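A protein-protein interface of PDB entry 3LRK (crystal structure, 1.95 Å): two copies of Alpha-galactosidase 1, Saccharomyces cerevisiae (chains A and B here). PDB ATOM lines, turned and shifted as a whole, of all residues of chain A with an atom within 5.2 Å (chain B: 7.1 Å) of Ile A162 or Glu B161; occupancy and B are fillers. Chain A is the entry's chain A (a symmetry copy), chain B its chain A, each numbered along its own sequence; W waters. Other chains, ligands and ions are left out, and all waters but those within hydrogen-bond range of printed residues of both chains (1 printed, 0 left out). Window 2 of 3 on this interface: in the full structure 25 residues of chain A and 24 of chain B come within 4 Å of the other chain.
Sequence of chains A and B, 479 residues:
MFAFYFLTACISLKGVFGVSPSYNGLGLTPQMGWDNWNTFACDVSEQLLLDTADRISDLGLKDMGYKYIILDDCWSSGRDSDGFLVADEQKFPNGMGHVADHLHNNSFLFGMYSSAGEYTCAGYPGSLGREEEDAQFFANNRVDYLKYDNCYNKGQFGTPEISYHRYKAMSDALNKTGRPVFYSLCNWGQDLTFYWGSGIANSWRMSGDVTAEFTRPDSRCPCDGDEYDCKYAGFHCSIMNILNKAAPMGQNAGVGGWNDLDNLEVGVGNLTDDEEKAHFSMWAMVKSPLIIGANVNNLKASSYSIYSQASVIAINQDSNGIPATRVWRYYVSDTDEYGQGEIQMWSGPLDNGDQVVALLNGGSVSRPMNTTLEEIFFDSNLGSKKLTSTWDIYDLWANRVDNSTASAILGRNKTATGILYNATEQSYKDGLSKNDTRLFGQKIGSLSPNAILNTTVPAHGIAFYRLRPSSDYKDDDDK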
ATOM      1  N   GLY A 155     -12.500  -5.765   7.906  1.00  0.00           N
ATOM      2  CA  GLY A 155     -12.372  -5.051   9.181  1.00  0.00           C
ATOM      3  C   GLY A 155     -13.584  -5.089  10.104  1.00  0.00           C
ATOM      4  O   GLY A 155     -13.576  -4.431  11.161  1.00  0.00           O
ATOM      5  N   GLN A 156     -14.594  -5.886   9.747  1.00  0.00           N
ATOM      6  CA  GLN A 156     -15.858  -5.927  10.513  1.00  0.00           C
ATOM      7  C   GLN A 156     -15.854  -6.962  11.641  1.00  0.00           C
ATOM      8  O   GLN A 156     -16.729  -7.836  11.732  1.00  0.00           O
ATOM      9  CB  GLN A 156     -17.061  -6.122   9.589  1.00  0.00           C
ATOM     10  CG  GLN A 156     -17.264  -5.003   8.590  1.00  0.00           C
ATOM     11  CD  GLN A 156     -18.562  -5.120   7.826  1.00  0.00           C
ATOM     12  OE1 GLN A 156     -19.526  -5.732   8.299  1.00  0.00           O
ATOM     13  NE2 GLN A 156     -18.605  -4.522   6.639  1.00  0.00           N
ATOM     14  N   PHE A 157     -14.857  -6.832  12.503  1.00  0.00           N
ATOM     15  CA  PHE A 157     -14.654  -7.685  13.663  1.00  0.00           C
ATOM     16  C   PHE A 157     -13.940  -6.842  14.726  1.00  0.00           C
ATOM     17  O   PHE A 157     -13.598  -5.679  14.466  1.00  0.00           O
ATOM     18  CB  PHE A 157     -13.827  -8.925  13.279  1.00  0.00           C
ATOM     19  CG  PHE A 157     -12.370  -8.638  13.057  1.00  0.00           C
ATOM     20  CD1 PHE A 157     -11.439  -8.904  14.063  1.00  0.00           C
ATOM     21  CD2 PHE A 157     -11.927  -8.086  11.853  1.00  0.00           C
ATOM     22  CE1 PHE A 157     -10.080  -8.623  13.877  1.00  0.00           C
ATOM     23  CE2 PHE A 157     -10.573  -7.802  11.651  1.00  0.00           C
ATOM     24  CZ  PHE A 157      -9.646  -8.069  12.674  1.00  0.00           C
ATOM     25  N   GLY A 158     -13.706  -7.414  15.905  1.00  0.00           N
ATOM     26  CA  GLY A 158     -12.900  -6.739  16.931  1.00  0.00           C
ATOM     27  C   GLY A 158     -13.648  -6.430  18.206  1.00  0.00           C
ATOM     28  O   GLY A 158     -13.046  -6.333  19.282  1.00  0.00           O
ATOM     29  N   THR A 159     -14.966  -6.303  18.089  1.00  0.00           N
ATOM     30  CA  THR A 159     -15.862  -6.200  19.243  1.00  0.00           C
ATOM     31  C   THR A 159     -17.037  -7.169  19.065  1.00  0.00           C
ATOM     32  O   THR A 159     -17.374  -7.536  17.946  1.00  0.00           O
ATOM     33  CB  THR A 159     -16.418  -4.763  19.437  1.00  0.00           C
ATOM     34  OG1 THR A 159     -17.314  -4.434  18.368  1.00  0.00           O
ATOM     35  CG2 THR A 159     -15.294  -3.713  19.517  1.00  0.00           C
ATOM     36  N   PRO A 160     -17.652  -7.621  20.174  1.00  0.00           N
ATOM     37  CA  PRO A 160     -18.888  -8.429  20.046  1.00  0.00           C
ATOM     38  C   PRO A 160     -19.955  -7.795  19.140  1.00  0.00           C
ATOM     39  O   PRO A 160     -20.551  -8.475  18.295  1.00  0.00           O
ATOM     40  CB  PRO A 160     -19.404  -8.485  21.491  1.00  0.00           C
ATOM     41  CG  PRO A 160     -18.147  -8.453  22.302  1.00  0.00           C
ATOM     42  CD  PRO A 160     -17.239  -7.470  21.578  1.00  0.00           C
ATOM     43  N   GLU A 161     -20.184  -6.500  19.301  1.00  0.00           N
ATOM     44  CA  GLU A 161     -21.273  -5.824  18.593  1.00  0.00           C
ATOM     45  C   GLU A 161     -21.112  -5.809  17.067  1.00  0.00           C
ATOM     46  O   GLU A 161     -22.082  -6.022  16.334  1.00  0.00           O
ATOM     47  CB  GLU A 161     -21.447  -4.409  19.136  1.00  0.00           C
ATOM     48  CG  GLU A 161     -22.619  -3.654  18.548  1.00  0.00           C
ATOM     49  CD  GLU A 161     -22.448  -2.151  18.658  1.00  0.00           C
ATOM     50  OE1 GLU A 161     -23.481  -1.459  18.779  1.00  0.00           O
ATOM     51  OE2 GLU A 161     -21.287  -1.659  18.615  1.00  0.00           O
ATOM     52  N   ILE A 162     -19.900  -5.529  16.588  1.00  0.00           N
ATOM     53  CA  ILE A 162     -19.661  -5.530  15.142  1.00  0.00           C
ATOM     54  C   ILE A 162     -19.769  -6.935  14.506  1.00  0.00           C
ATOM     55  O   ILE A 162     -20.337  -7.078  13.426  1.00  0.00           O
ATOM     56  CB  ILE A 162     -18.331  -4.819  14.750  1.00  0.00           C
ATOM     57  CG1 ILE A 162     -18.262  -4.634  13.230  1.00  0.00           C
ATOM     58  CG2 ILE A 162     -17.106  -5.579  15.286  1.00  0.00           C
ATOM     59  CD1 ILE A 162     -17.263  -3.558  12.773  1.00  0.00           C
ATOM     60  N   SER A 163     -19.225  -7.956  15.168  1.00  0.00           N
ATOM     61  CA  SER A 163     -19.310  -9.327  14.641  1.00  0.00           C
ATOM     62  C   SER A 163     -20.750  -9.855  14.706  1.00  0.00           C
ATOM     63  O   SER A 163     -21.236 -10.503  13.772  1.00  0.00           O
ATOM     64  CB  SER A 163     -18.363 -10.254  15.396  1.00  0.00           C
ATOM     65  OG  SER A 163     -17.027 -10.024  14.987  1.00  0.00           O
ATOM     66  N   TYR A 164     -21.430  -9.572  15.812  1.00  0.00           N
ATOM     67  CA  TYR A 164     -22.841  -9.905  15.940  1.00  0.00           C
ATOM     68  C   TYR A 164     -23.695  -9.309  14.812  1.00  0.00           C
ATOM     69  O   TYR A 164     -24.514 -10.005  14.228  1.00  0.00           O
ATOM     70  CB  TYR A 164     -23.371  -9.438  17.301  1.00  0.00           C
ATOM     71  CG  TYR A 164     -24.875  -9.464  17.419  1.00  0.00           C
ATOM     72  CD1 TYR A 164     -25.550 -10.643  17.778  1.00  0.00           C
ATOM     73  CD2 TYR A 164     -25.627  -8.312  17.186  1.00  0.00           C
ATOM     74  CE1 TYR A 164     -26.922 -10.662  17.904  1.00  0.00           C
ATOM     75  CE2 TYR A 164     -27.013  -8.322  17.298  1.00  0.00           C
ATOM     76  CZ  TYR A 164     -27.652  -9.501  17.663  1.00  0.00           C
ATOM     77  OH  TYR A 164     -29.029  -9.521  17.784  1.00  0.00           O
ATOM     78  N   HIS A 165     -23.521  -8.024  14.511  1.00  0.00           N
ATOM     79  CA  HIS A 165     -24.342  -7.407  13.466  1.00  0.00           C
ATOM     80  C   HIS A 165     -24.057  -7.981  12.070  1.00  0.00           C
ATOM     81  O   HIS A 165     -24.980  -8.159  11.273  1.00  0.00           O
ATOM     82  CB  HIS A 165     -24.262  -5.884  13.521  1.00  0.00           C
ATOM     83  CG  HIS A 165     -25.127  -5.293  14.600  1.00  0.00           C
ATOM     84  ND1 HIS A 165     -26.502  -5.411  14.596  1.00  0.00           N
ATOM     85  CD2 HIS A 165     -24.814  -4.615  15.731  1.00  0.00           C
ATOM     86  CE1 HIS A 165     -26.999  -4.811  15.665  1.00  0.00           C
ATOM     87  NE2 HIS A 165     -25.995  -4.331  16.374  1.00  0.00           N
ATOM     88  N   ARG A 166     -22.800  -8.337  11.809  1.00  0.00           N
ATOM     89  CA  ARG A 166     -22.420  -8.969  10.527  1.00  0.00           C
ATOM     90  C   ARG A 166     -23.073 -10.354  10.361  1.00  0.00           C
ATOM     91  O   ARG A 166     -23.600 -10.678   9.284  1.00  0.00           O
ATOM     92  CB  ARG A 166     -20.890  -9.067  10.395  1.00  0.00           C
ATOM     93  CG  ARG A 166     -20.372  -9.737   9.082  1.00  0.00           C
ATOM     94  CD  ARG A 166     -18.914  -9.346   8.753  1.00  0.00           C
ATOM     95  NE  ARG A 166     -18.056  -9.539   9.917  1.00  0.00           N
ATOM     96  CZ  ARG A 166     -17.471 -10.674  10.258  1.00  0.00           C
ATOM     97  NH1 ARG A 166     -17.563 -11.763   9.477  1.00  0.00           N
ATOM     98  NH2 ARG A 166     -16.771 -10.723  11.387  1.00  0.00           N
ATOM     99  N   ASP A 191     -14.495 -12.634  19.043  1.00  0.00           N
ATOM    100  CA  ASP A 191     -15.338 -11.652  19.724  1.00  0.00           C
ATOM    101  C   ASP A 191     -16.407 -12.301  20.635  1.00  0.00           C
ATOM    102  O   ASP A 191     -17.509 -11.779  20.758  1.00  0.00           O
ATOM    103  CB  ASP A 191     -15.966 -10.671  18.707  1.00  0.00           C
ATOM    104  CG  ASP A 191     -14.906  -9.893  17.929  1.00  0.00           C
ATOM    105  OD1 ASP A 191     -13.892  -9.503  18.538  1.00  0.00           O
ATOM    106  OD2 ASP A 191     -15.089  -9.686  16.728  1.00  0.00           O
ATOM    107  N   GLY B 158      -7.336   1.558  17.822  1.00  0.00           N
ATOM    108  CA  GLY B 158      -7.823   0.899  19.041  1.00  0.00           C
ATOM    109  C   GLY B 158      -8.743  -0.272  18.787  1.00  0.00           C
ATOM    110  O   GLY B 158      -8.836  -1.190  19.612  1.00  0.00           O
ATOM    111  N   THR B 159      -9.403  -0.253  17.633  1.00  0.00           N
ATOM    112  CA  THR B 159     -10.179  -1.392  17.141  1.00  0.00           C
ATOM    113  C   THR B 159      -9.817  -1.662  15.676  1.00  0.00           C
ATOM    114  O   THR B 159      -9.363  -0.766  14.974  1.00  0.00           O
ATOM    115  CB  THR B 159     -11.711  -1.158  17.247  1.00  0.00           C
ATOM    116  OG1 THR B 159     -12.116  -0.136  16.326  1.00  0.00           O
ATOM    117  CG2 THR B 159     -12.142  -0.775  18.674  1.00  0.00           C
ATOM    118  N   PRO B 160      -9.979  -2.914  15.208  1.00  0.00           N
ATOM    119  CA  PRO B 160      -9.795  -3.184  13.761  1.00  0.00           C
ATOM    120  C   PRO B 160     -10.579  -2.232  12.846  1.00  0.00           C
ATOM    121  O   PRO B 160     -10.040  -1.722  11.855  1.00  0.00           O
ATOM    122  CB  PRO B 160     -10.342  -4.612  13.614  1.00  0.00           C
ATOM    123  CG  PRO B 160     -10.024  -5.236  14.937  1.00  0.00           C
ATOM    124  CD  PRO B 160     -10.287  -4.142  15.960  1.00  0.00           C
ATOM    125  N   GLU B 161     -11.837  -1.980  13.181  1.00  0.00           N
ATOM    126  CA  GLU B 161     -12.717  -1.202  12.306  1.00  0.00           C
ATOM    127  C   GLU B 161     -12.271   0.252  12.104  1.00  0.00           C
ATOM    128  O   GLU B 161     -12.327   0.772  10.986  1.00  0.00           O
ATOM    129  CB  GLU B 161     -14.150  -1.264  12.825  1.00  0.00           C
ATOM    130  CG  GLU B 161     -15.167  -0.581  11.935  1.00  0.00           C
ATOM    131  CD  GLU B 161     -16.415  -0.173  12.697  1.00  0.00           C
ATOM    132  OE1 GLU B 161     -17.495  -0.163  12.069  1.00  0.00           O
ATOM    133  OE2 GLU B 161     -16.316   0.146  13.913  1.00  0.00           O
ATOM    134  N   ILE B 162     -11.857   0.915  13.183  1.00  0.00           N
ATOM    135  CA  ILE B 162     -11.383   2.298  13.061  1.00  0.00           C
ATOM    136  C   ILE B 162     -10.059   2.421  12.275  1.00  0.00           C
ATOM    137  O   ILE B 162      -9.910   3.331  11.462  1.00  0.00           O
ATOM    138  CB  ILE B 162     -11.311   3.033  14.434  1.00  0.00           C
ATOM    139  CG1 ILE B 162     -11.052   4.527  14.214  1.00  0.00           C
ATOM    140  CG2 ILE B 162     -10.253   2.403  15.356  1.00  0.00           C
ATOM    141  CD1 ILE B 162     -11.423   5.411  15.417  1.00  0.00           C
ATOM    142  N   SER B 163      -9.108   1.518  12.517  1.00  0.00           N
ATOM    143  CA  SER B 163      -7.830   1.553  11.788  1.00  0.00           C
ATOM    144  C   SER B 163      -8.026   1.175  10.314  1.00  0.00           C
ATOM    145  O   SER B 163      -7.443   1.788   9.412  1.00  0.00           O
ATOM    146  CB  SER B 163      -6.808   0.634  12.448  1.00  0.00           C
ATOM    147  OG  SER B 163      -6.314   1.229  13.635  1.00  0.00           O
ATOM    148  N   TYR B 164      -8.850   0.160  10.071  1.00  0.00           N
ATOM    149  CA  TYR B 164      -9.217  -0.212   8.713  1.00  0.00           C
ATOM    150  C   TYR B 164      -9.818   0.959   7.921  1.00  0.00           C
ATOM    151  O   TYR B 164      -9.430   1.195   6.785  1.00  0.00           O
ATOM    152  CB  TYR B 164     -10.198  -1.389   8.735  1.00  0.00           C
ATOM    153  CG  TYR B 164     -10.867  -1.659   7.411  1.00  0.00           C
ATOM    154  CD1 TYR B 164     -10.240  -2.452   6.435  1.00  0.00           C
ATOM    155  CD2 TYR B 164     -12.131  -1.137   7.133  1.00  0.00           C
ATOM    156  CE1 TYR B 164     -10.860  -2.715   5.232  1.00  0.00           C
ATOM    157  CE2 TYR B 164     -12.760  -1.385   5.916  1.00  0.00           C
ATOM    158  CZ  TYR B 164     -12.119  -2.180   4.974  1.00  0.00           C
ATOM    159  OH  TYR B 164     -12.738  -2.438   3.766  1.00  0.00           O
ATOM    160  N   HIS B 165     -10.771   1.681   8.504  1.00  0.00           N
ATOM    161  CA  HIS B 165     -11.398   2.782   7.769  1.00  0.00           C
ATOM    162  C   HIS B 165     -10.422   3.933   7.478  1.00  0.00           C
ATOM    163  O   HIS B 165     -10.472   4.530   6.401  1.00  0.00           O
ATOM    164  CB  HIS B 165     -12.688   3.239   8.442  1.00  0.00           C
ATOM    165  CG  HIS B 165     -13.853   2.334   8.149  1.00  0.00           C
ATOM    166  ND1 HIS B 165     -14.355   2.161   6.876  1.00  0.00           N
ATOM    167  CD2 HIS B 165     -14.586   1.526   8.953  1.00  0.00           C
ATOM    168  CE1 HIS B 165     -15.362   1.305   6.912  1.00  0.00           C
ATOM    169  NE2 HIS B 165     -15.515   0.897   8.158  1.00  0.00           N
ATOM    170  N   ARG B 166      -9.497   4.187   8.401  1.00  0.00           N
ATOM    171  CA  ARG B 166      -8.458   5.222   8.200  1.00  0.00           C
ATOM    172  C   ARG B 166      -7.511   4.855   7.042  1.00  0.00           C
ATOM    173  O   ARG B 166      -7.189   5.708   6.197  1.00  0.00           O
ATOM    174  CB  ARG B 166      -7.668   5.467   9.496  1.00  0.00           C
ATOM    175  CG  ARG B 166      -6.528   6.531   9.395  1.00  0.00           C
ATOM    176  CD  ARG B 166      -6.140   7.115  10.772  1.00  0.00           C
ATOM    177  NE  ARG B 166      -5.893   6.045  11.733  1.00  0.00           N
ATOM    178  CZ  ARG B 166      -4.745   5.411  11.894  1.00  0.00           C
ATOM    179  NH1 ARG B 166      -3.649   5.776  11.209  1.00  0.00           N
ATOM    180  NH2 ARG B 166      -4.683   4.405  12.761  1.00  0.00           N
ATOM    181  N   ASP B 191      -3.986  -3.184  15.823  1.00  0.00           N
ATOM    182  CA  ASP B 191      -5.376  -3.586  15.607  1.00  0.00           C
ATOM    183  C   ASP B 191      -5.519  -4.762  14.612  1.00  0.00           C
ATOM    184  O   ASP B 191      -6.486  -4.817  13.860  1.00  0.00           O
ATOM    185  CB  ASP B 191      -6.238  -2.371  15.192  1.00  0.00           C
ATOM    186  CG  ASP B 191      -6.244  -1.278  16.259  1.00  0.00           C
ATOM    187  OD1 ASP B 191      -6.289  -1.620  17.456  1.00  0.00           O
ATOM    188  OD2 ASP B 191      -6.196  -0.100  15.898  1.00  0.00           O
ATOM    189  N   TRP B 196      -7.144  -7.552   8.031  1.00  0.00           N
ATOM    190  CA  TRP B 196      -7.862  -6.594   7.172  1.00  0.00           C
ATOM    191  C   TRP B 196      -7.037  -5.883   6.086  1.00  0.00           C
ATOM    192  O   TRP B 196      -7.582  -5.134   5.275  1.00  0.00           O
ATOM    193  CB  TRP B 196      -8.618  -5.554   8.016  1.00  0.00           C
ATOM    194  CG  TRP B 196      -7.805  -4.854   9.113  1.00  0.00           C
ATOM    195  CD1 TRP B 196      -7.755  -5.195  10.430  1.00  0.00           C
ATOM    196  CD2 TRP B 196      -6.980  -3.692   8.968  1.00  0.00           C
ATOM    197  NE1 TRP B 196      -6.952  -4.312  11.127  1.00  0.00           N
ATOM    198  CE2 TRP B 196      -6.449  -3.392  10.248  1.00  0.00           C
ATOM    199  CE3 TRP B 196      -6.627  -2.876   7.879  1.00  0.00           C
ATOM    200  CZ2 TRP B 196      -5.582  -2.307  10.471  1.00  0.00           C
ATOM    201  CZ3 TRP B 196      -5.766  -1.798   8.104  1.00  0.00           C
ATOM    202  CH2 TRP B 196      -5.263  -1.523   9.392  1.00  0.00           C
HETATM  203  O   HOH W   1     -13.509  -3.173  15.284  1.00  0.00           O
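Gly A158 touches Pro B160, but with the chains exchanged Pro A160 does not touch Gly B158 (10.7 Å).
Ile A162 touches Glu B161, but with the chains exchanged Glu A161 does not touch Ile B162 (11.2 Å).
Positions printed for both chains: 158, 159, 160, 161, 162, 163, 164, 165, 166 and 191.
Of the 5 pairs that touch across the chains among the printed residues, none has its exchanged pair printed and touching as well.
Of the printed residues of chain B, Gly A155 touches Glu B161 and Trp B196.
Printed residues of chain B within 4 Å of Phe A157: Pro B160 (3.5 Å).
Pro A160 touches none of the printed residues of chain B.
Of chain B, only Glu B161 comes within 4 Å of Ile A162.
Of the printed residues of chain A, Pro B160 touches Phe A157 and Gly A158.
Glu B161 touches just these residues of chain A: Gly A155 (3.5 Å) and Ile A162 (3.5 Å).
Ile B162 touches none of the printed residues of chain A.
The nearest printed residue of chain B that does not touch Phe A157 is Trp B196 (4.03 Å).
Hydrophobic or aromatic side chains of chain A within 4 Å of the printed part of chain B: Phe A157 and Ile A162.
Of the 11 printed residues of chain B, 3 touch a printed residue of chain A.
Hydrophobic or aromatic side chains of chain B within 4 Å of the printed part of chain A: Pro B160 and Trp B196.
Along chain B the printed residues that touch a printed residue of chain A span positions 160 to 196.
Among the printed residues, 5 pairs touch across the chains.
Among the printed residues, no Asp or Glu carboxylate lies within 4 Å of a Lys or Arg side-chain nitrogen of the other chain.
The indole nitrogen (NE1) of Trp B196 lies within hydrogen-bond range of the backbone carbonyl oxygen (O) of Asp B191 (2.8 Å).
OD2 of Asp A191 lies within hydrogen-bond range of N of Gly A158, 2.8 Å away.
The backbone NH (N) of Ile A162 lies close to the side-chain hydroxyl (OG1) of Thr A159 (3.3 Å).
Gly A155 touches Glu B161 (O to CA, 3.5 Å).
Trp B196 touches Gly A155.
CB of Pro B160 touches O of Phe A157, at 3.5 Å.
CA of Gly A158 touches CG of Pro B160, at 3.8 Å.
Ile A162 touches Glu B161 (CD1 to OE1, 3.5 Å).
Water W1 lies within hydrogen-bond range of O of Phe A157, N of Glu B161 and OG1 of Thr B159.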
